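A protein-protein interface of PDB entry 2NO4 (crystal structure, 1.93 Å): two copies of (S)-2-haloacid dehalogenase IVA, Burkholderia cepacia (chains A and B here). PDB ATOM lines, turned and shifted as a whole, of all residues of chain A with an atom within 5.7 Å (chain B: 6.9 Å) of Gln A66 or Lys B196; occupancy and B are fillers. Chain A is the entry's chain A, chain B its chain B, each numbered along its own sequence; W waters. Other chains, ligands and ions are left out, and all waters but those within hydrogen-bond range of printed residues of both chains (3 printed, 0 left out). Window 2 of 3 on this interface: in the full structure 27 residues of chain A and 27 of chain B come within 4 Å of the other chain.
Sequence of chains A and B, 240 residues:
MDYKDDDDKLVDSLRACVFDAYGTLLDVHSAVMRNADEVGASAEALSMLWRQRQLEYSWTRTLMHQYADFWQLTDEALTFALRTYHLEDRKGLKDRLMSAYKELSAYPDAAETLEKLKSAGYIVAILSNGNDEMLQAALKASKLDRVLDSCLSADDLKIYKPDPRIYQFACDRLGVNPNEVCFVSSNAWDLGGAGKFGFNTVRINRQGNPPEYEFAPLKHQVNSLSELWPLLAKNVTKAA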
ATOM      1  N   ARG A  61      27.280  12.012   7.943  1.00  0.00           N
ATOM      2  CA  ARG A  61      25.891  12.038   7.480  1.00  0.00           C
ATOM      3  C   ARG A  61      24.914  11.656   8.589  1.00  0.00           C
ATOM      4  O   ARG A  61      23.790  12.119   8.607  1.00  0.00           O
ATOM      5  CB  ARG A  61      25.670  11.113   6.294  1.00  0.00           C
ATOM      6  CG  ARG A  61      26.068  11.735   4.929  1.00  0.00           C
ATOM      7  CD  ARG A  61      25.978  10.613   3.930  1.00  0.00           C
ATOM      8  NE  ARG A  61      26.072  10.982   2.529  1.00  0.00           N
ATOM      9  CZ  ARG A  61      25.043  11.306   1.743  1.00  0.00           C
ATOM     10  NH1 ARG A  61      23.798  11.413   2.209  1.00  0.00           N
ATOM     11  NH2 ARG A  61      25.284  11.572   0.479  1.00  0.00           N
ATOM     12  N   THR A  62      25.337  10.794   9.502  1.00  0.00           N
ATOM     13  CA  THR A  62      24.484  10.473  10.653  1.00  0.00           C
ATOM     14  C   THR A  62      24.347  11.689  11.587  1.00  0.00           C
ATOM     15  O   THR A  62      23.245  12.047  11.996  1.00  0.00           O
ATOM     16  CB  THR A  62      25.039   9.275  11.442  1.00  0.00           C
ATOM     17  OG1 THR A  62      25.053   8.144  10.594  1.00  0.00           O
ATOM     18  CG2 THR A  62      24.104   8.901  12.669  1.00  0.00           C
ATOM     19  N   MET A  64      24.595  14.822  10.815  1.00  0.00           N
ATOM     20  CA  MET A  64      23.866  15.903  10.227  1.00  0.00           C
ATOM     21  C   MET A  64      22.464  15.475   9.756  1.00  0.00           C
ATOM     22  O   MET A  64      21.730  16.283   9.207  1.00  0.00           O
ATOM     23  CB  MET A  64      24.713  16.597   9.118  1.00  0.00           C
ATOM     24  CG  MET A  64      24.732  15.829   7.783  1.00  0.00           C
ATOM     25  SD  MET A  64      25.701  16.763   6.537  1.00  0.00           S
ATOM     26  CE  MET A  64      27.383  16.400   6.882  1.00  0.00           C
ATOM     27  N   HIS A  65      22.099  14.212   9.991  1.00  0.00           N
ATOM     28  CA  HIS A  65      20.756  13.699   9.659  1.00  0.00           C
ATOM     29  C   HIS A  65      20.494  13.659   8.138  1.00  0.00           C
ATOM     30  O   HIS A  65      19.411  14.018   7.678  1.00  0.00           O
ATOM     31  CB  HIS A  65      19.628  14.422  10.452  1.00  0.00           C
ATOM     32  CG  HIS A  65      19.920  14.546  11.921  1.00  0.00           C
ATOM     33  ND1 HIS A  65      19.746  13.506  12.803  1.00  0.00           N
ATOM     34  CD2 HIS A  65      20.391  15.582  12.658  1.00  0.00           C
ATOM     35  CE1 HIS A  65      20.114  13.887  14.020  1.00  0.00           C
ATOM     36  NE2 HIS A  65      20.520  15.141  13.955  1.00  0.00           N
ATOM     37  N   GLN A  66      21.503  13.251   7.367  1.00  0.00           N
ATOM     38  CA  GLN A  66      21.305  13.078   5.927  1.00  0.00           C
ATOM     39  C   GLN A  66      21.814  11.674   5.550  1.00  0.00           C
ATOM     40  O   GLN A  66      22.765  11.525   4.790  1.00  0.00           O
ATOM     41  CB  GLN A  66      22.072  14.158   5.148  1.00  0.00           C
ATOM     42  CG  GLN A  66      21.831  14.114   3.626  1.00  0.00           C
ATOM     43  CD  GLN A  66      20.499  14.724   3.193  1.00  0.00           C
ATOM     44  OE1 GLN A  66      19.857  15.477   3.952  1.00  0.00           O
ATOM     45  NE2 GLN A  66      20.055  14.374   1.973  1.00  0.00           N
ATOM     46  N   TYR A  67      21.144  10.651   6.055  1.00  0.00           N
ATOM     47  CA  TYR A  67      21.474   9.259   5.718  1.00  0.00           C
ATOM     48  C   TYR A  67      21.309   8.919   4.233  1.00  0.00           C
ATOM     49  O   TYR A  67      20.323   9.335   3.580  1.00  0.00           O
ATOM     50  CB  TYR A  67      20.576   8.318   6.562  1.00  0.00           C
ATOM     51  CG  TYR A  67      20.803   6.843   6.269  1.00  0.00           C
ATOM     52  CD1 TYR A  67      21.783   6.134   6.960  1.00  0.00           C
ATOM     53  CD2 TYR A  67      20.104   6.194   5.242  1.00  0.00           C
ATOM     54  CE1 TYR A  67      22.048   4.782   6.681  1.00  0.00           C
ATOM     55  CE2 TYR A  67      20.345   4.829   4.964  1.00  0.00           C
ATOM     56  CZ  TYR A  67      21.328   4.147   5.713  1.00  0.00           C
ATOM     57  OH  TYR A  67      21.592   2.823   5.492  1.00  0.00           O
ATOM     58  N   ALA A  68      22.266   8.131   3.712  1.00  0.00           N
ATOM     59  CA  ALA A  68      22.123   7.399   2.458  1.00  0.00           C
ATOM     60  C   ALA A  68      22.789   6.073   2.767  1.00  0.00           C
ATOM     61  O   ALA A  68      23.648   6.028   3.648  1.00  0.00           O
ATOM     62  CB  ALA A  68      22.838   8.140   1.276  1.00  0.00           C
ATOM     63  N   PRO B 164      23.652  19.550  13.888  1.00  0.00           N
ATOM     64  CA  PRO B 164      23.044  20.880  13.747  1.00  0.00           C
ATOM     65  C   PRO B 164      23.020  21.745  15.025  1.00  0.00           C
ATOM     66  O   PRO B 164      22.983  22.975  14.901  1.00  0.00           O
ATOM     67  CB  PRO B 164      21.627  20.570  13.261  1.00  0.00           C
ATOM     68  CG  PRO B 164      21.367  19.074  13.740  1.00  0.00           C
ATOM     69  CD  PRO B 164      22.709  18.476  13.512  1.00  0.00           C
ATOM     70  N   ASP B 190      31.869  20.128   7.063  1.00  0.00           N
ATOM     71  CA  ASP B 190      31.451  21.283   7.834  1.00  0.00           C
ATOM     72  C   ASP B 190      30.523  22.146   6.970  1.00  0.00           C
ATOM     73  O   ASP B 190      29.476  22.597   7.445  1.00  0.00           O
ATOM     74  CB  ASP B 190      32.711  22.048   8.260  1.00  0.00           C
ATOM     75  CG  ASP B 190      32.437  23.183   9.263  1.00  0.00           C
ATOM     76  OD1 ASP B 190      31.365  23.203   9.927  1.00  0.00           O
ATOM     77  OD2 ASP B 190      33.348  24.058   9.374  1.00  0.00           O
ATOM     78  N   LEU B 191      30.885  22.355   5.707  1.00  0.00           N
ATOM     79  CA  LEU B 191      29.973  22.989   4.725  1.00  0.00           C
ATOM     80  C   LEU B 191      28.679  22.163   4.531  1.00  0.00           C
ATOM     81  O   LEU B 191      27.618  22.725   4.378  1.00  0.00           O
ATOM     82  CB  LEU B 191      30.666  23.255   3.377  1.00  0.00           C
ATOM     83  CG  LEU B 191      31.902  24.167   3.514  1.00  0.00           C
ATOM     84  CD1 LEU B 191      32.888  23.834   2.407  1.00  0.00           C
ATOM     85  CD2 LEU B 191      31.511  25.649   3.536  1.00  0.00           C
ATOM     86  N   GLY B 192      28.797  20.840   4.499  1.00  0.00           N
ATOM     87  CA  GLY B 192      27.633  19.968   4.395  1.00  0.00           C
ATOM     88  C   GLY B 192      26.686  20.170   5.560  1.00  0.00           C
ATOM     89  O   GLY B 192      25.509  20.395   5.345  1.00  0.00           O
ATOM     90  N   GLY B 193      27.224  20.142   6.790  1.00  0.00           N
ATOM     91  CA  GLY B 193      26.430  20.367   7.988  1.00  0.00           C
ATOM     92  C   GLY B 193      25.810  21.754   8.080  1.00  0.00           C
ATOM     93  O   GLY B 193      24.612  21.873   8.371  1.00  0.00           O
ATOM     94  N   ALA B 194      26.627  22.789   7.833  1.00  0.00           N
ATOM     95  CA  ALA B 194      26.200  24.184   7.851  1.00  0.00           C
ATOM     96  C   ALA B 194      25.152  24.488   6.785  1.00  0.00           C
ATOM     97  O   ALA B 194      24.190  25.225   7.037  1.00  0.00           O
ATOM     98  CB  ALA B 194      27.447  25.114   7.652  1.00  0.00           C
ATOM     99  N   GLY B 195      25.334  23.920   5.607  1.00  0.00           N
ATOM    100  CA  GLY B 195      24.427  24.126   4.458  1.00  0.00           C
ATOM    101  C   GLY B 195      23.093  23.450   4.706  1.00  0.00           C
ATOM    102  O   GLY B 195      22.013  24.064   4.511  1.00  0.00           O
ATOM    103  N   LYS B 196      23.147  22.197   5.165  1.00  0.00           N
ATOM    104  CA  LYS B 196      21.912  21.496   5.564  1.00  0.00           C
ATOM    105  C   LYS B 196      21.168  22.217   6.693  1.00  0.00           C
ATOM    106  O   LYS B 196      19.955  22.334   6.643  1.00  0.00           O
ATOM    107  CB  LYS B 196      22.161  20.052   5.939  1.00  0.00           C
ATOM    108  CG  LYS B 196      20.851  19.260   5.956  1.00  0.00           C
ATOM    109  CD  LYS B 196      21.086  17.860   6.347  1.00  0.00           C
ATOM    110  CE  LYS B 196      19.817  17.332   6.999  1.00  0.00           C
ATOM    111  NZ  LYS B 196      18.799  17.124   5.954  1.00  0.00           N
ATOM    112  N   PHE B 197      21.891  22.723   7.681  1.00  0.00           N
ATOM    113  CA  PHE B 197      21.305  23.567   8.722  1.00  0.00           C
ATOM    114  C   PHE B 197      20.625  24.835   8.167  1.00  0.00           C
ATOM    115  O   PHE B 197      19.589  25.291   8.702  1.00  0.00           O
ATOM    116  CB  PHE B 197      22.367  23.932   9.785  1.00  0.00           C
ATOM    117  CG  PHE B 197      21.841  24.845  10.866  1.00  0.00           C
ATOM    118  CD1 PHE B 197      21.063  24.322  11.901  1.00  0.00           C
ATOM    119  CD2 PHE B 197      22.099  26.216  10.825  1.00  0.00           C
ATOM    120  CE1 PHE B 197      20.518  25.150  12.900  1.00  0.00           C
ATOM    121  CE2 PHE B 197      21.588  27.062  11.816  1.00  0.00           C
ATOM    122  CZ  PHE B 197      20.780  26.526  12.850  1.00  0.00           C
ATOM    123  N   GLY B 198      21.180  25.415   7.103  1.00  0.00           N
ATOM    124  CA  GLY B 198      20.583  26.625   6.518  1.00  0.00           C
ATOM    125  C   GLY B 198      21.461  27.864   6.373  1.00  0.00           C
ATOM    126  O   GLY B 198      20.979  28.897   5.893  1.00  0.00           O
ATOM    127  N   PHE B 199      22.733  27.792   6.782  1.00  0.00           N
ATOM    128  CA  PHE B 199      23.658  28.930   6.536  1.00  0.00           C
ATOM    129  C   PHE B 199      23.947  29.034   5.051  1.00  0.00           C
ATOM    130  O   PHE B 199      23.844  28.048   4.362  1.00  0.00           O
ATOM    131  CB  PHE B 199      25.001  28.734   7.215  1.00  0.00           C
ATOM    132  CG  PHE B 199      24.974  28.835   8.715  1.00  0.00           C
ATOM    133  CD1 PHE B 199      23.933  29.480   9.389  1.00  0.00           C
ATOM    134  CD2 PHE B 199      26.026  28.294   9.453  1.00  0.00           C
ATOM    135  CE1 PHE B 199      23.944  29.592  10.821  1.00  0.00           C
ATOM    136  CE2 PHE B 199      26.064  28.388  10.866  1.00  0.00           C
ATOM    137  CZ  PHE B 199      25.014  29.064  11.548  1.00  0.00           C
ATOM    138  N   THR B 201      26.604  28.982   2.419  1.00  0.00           N
ATOM    139  CA  THR B 201      27.932  28.376   2.530  1.00  0.00           C
ATOM    140  C   THR B 201      28.897  28.788   1.429  1.00  0.00           C
ATOM    141  O   THR B 201      28.548  28.839   0.255  1.00  0.00           O
ATOM    142  CB  THR B 201      27.841  26.831   2.620  1.00  0.00           C
ATOM    143  OG1 THR B 201      27.027  26.364   1.543  1.00  0.00           O
ATOM    144  CG2 THR B 201      27.192  26.448   3.949  1.00  0.00           C
ATOM    145  N   PHE B 215      24.316  17.080  -1.667  1.00  0.00           N
ATOM    146  CA  PHE B 215      22.952  17.346  -1.152  1.00  0.00           C
ATOM    147  C   PHE B 215      22.849  18.701  -0.434  1.00  0.00           C
ATOM    148  O   PHE B 215      21.761  19.171  -0.229  1.00  0.00           O
ATOM    149  CB  PHE B 215      22.458  16.222  -0.218  1.00  0.00           C
ATOM    150  CG  PHE B 215      23.340  16.028   0.984  1.00  0.00           C
ATOM    151  CD1 PHE B 215      23.222  16.865   2.084  1.00  0.00           C
ATOM    152  CD2 PHE B 215      24.366  15.079   0.968  1.00  0.00           C
ATOM    153  CE1 PHE B 215      24.107  16.701   3.187  1.00  0.00           C
ATOM    154  CE2 PHE B 215      25.243  14.920   2.072  1.00  0.00           C
ATOM    155  CZ  PHE B 215      25.116  15.706   3.142  1.00  0.00           C
ATOM    156  N   ALA B 216      23.969  19.314  -0.035  1.00  0.00           N
ATOM    157  CA  ALA B 216      23.936  20.646   0.549  1.00  0.00           C
ATOM    158  C   ALA B 216      24.779  21.587  -0.329  1.00  0.00           C
ATOM    159  O   ALA B 216      25.976  21.845  -0.038  1.00  0.00           O
ATOM    160  CB  ALA B 216      24.421  20.654   2.047  1.00  0.00           C
ATOM    161  N   PRO B 217      24.163  22.116  -1.414  1.00  0.00           N
ATOM    162  CA  PRO B 217      24.961  22.921  -2.355  1.00  0.00           C
ATOM    163  C   PRO B 217      25.576  24.177  -1.726  1.00  0.00           C
ATOM    164  O   PRO B 217      24.980  24.812  -0.833  1.00  0.00           O
ATOM    165  CB  PRO B 217      23.943  23.356  -3.432  1.00  0.00           C
ATOM    166  CG  PRO B 217      22.719  22.551  -3.200  1.00  0.00           C
ATOM    167  CD  PRO B 217      22.745  22.019  -1.810  1.00  0.00           C
HETATM  168  O   HOH W   1      16.735  15.009   4.433  1.00  0.00           O
HETATM  169  O   HOH W   2      16.905  15.800   7.921  1.00  0.00           O
HETATM  170  O   HOH W   3      18.853  17.998   2.812  1.00  0.00           O
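SD of Met A64 lies within hydrogen-bond range of N of Gly B193 (3.7 Å).
OE1 of Gln A66 sits at hydrogen-bond distance from NZ of Lys B196, at 2.8 Å.
O of Gln A66 lies within hydrogen-bond range of NH1 of Arg A61 (2.8 Å).
Among the printed residues, merely in contact across the chains: Arg A61 with Phe B215 (3.6 Å), Met A64 with Gly B192 (3.7 Å), Met A64 with Lys B196 (3.1 Å), Met A64 with Phe B215 (3.6 Å), His A65 with Pro B164 (3.8 Å), His A65 with Lys B196 (3.4 Å) and Gln A66 with Phe B215 (3.4 Å).
Of the printed residues of chain B, Arg A61 touches Phe B215.
Of the printed residues of chain B, His A65 touches Pro B164 and Lys B196.
Gln A66 touches just these residues of chain B: Lys B196 (2.8 Å) and Phe B215 (3.4 Å).
Of the printed residues of chain A, Pro B164 touches His A65.
Asp B190 touches none of the printed residues of chain A.
Printed residues of chain A within 4 Å of Gly B192: Met A64.
Lys B196 touches just these residues of chain A: Met A64, His A65 and Gln A66.
Thr B201 touches none of the printed residues of chain A.
Of the printed residues of chain A, Phe B215 touches Arg A61 (3.6 Å), Met A64 (3.6 Å) and Gln A66 (3.4 Å).
The nearest residue of chain B that does not touch Gln A66 is Ala B216 (6.6 Å).
Of the 15 printed residues of chain B, 5 touch a printed residue of chain A.
Hydrophobic or aromatic side chains of chain B that line the printed part of chain A: Pro B164 and Phe B215.
Along chain B the printed residues that touch a printed residue of chain A span positions 164 to 215.
Hydrophobic or aromatic side chains of chain A within 4 Å of the printed part of chain B: Met A64 and His A65.
No position is printed for both chains.
Of the 9 pairs that touch across the chains among the printed residues, none has its exchanged pair printed and touching as well.
Water W3 bridges the side-chain amide oxygen of Gln A66 (2.9 Å) and the side-chain amino group of Lys B196 (3.3 Å).
Water W2 bridges the side-chain amino group of Lys B196 (3.0 Å) and the backbone carbonyl oxygen of His A65 (3.1 Å).
Water W1 bridges the side-chain amide oxygen of Gln A66 (3.2 Å) and the side-chain amino group of Lys B196 (3.3 Å).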
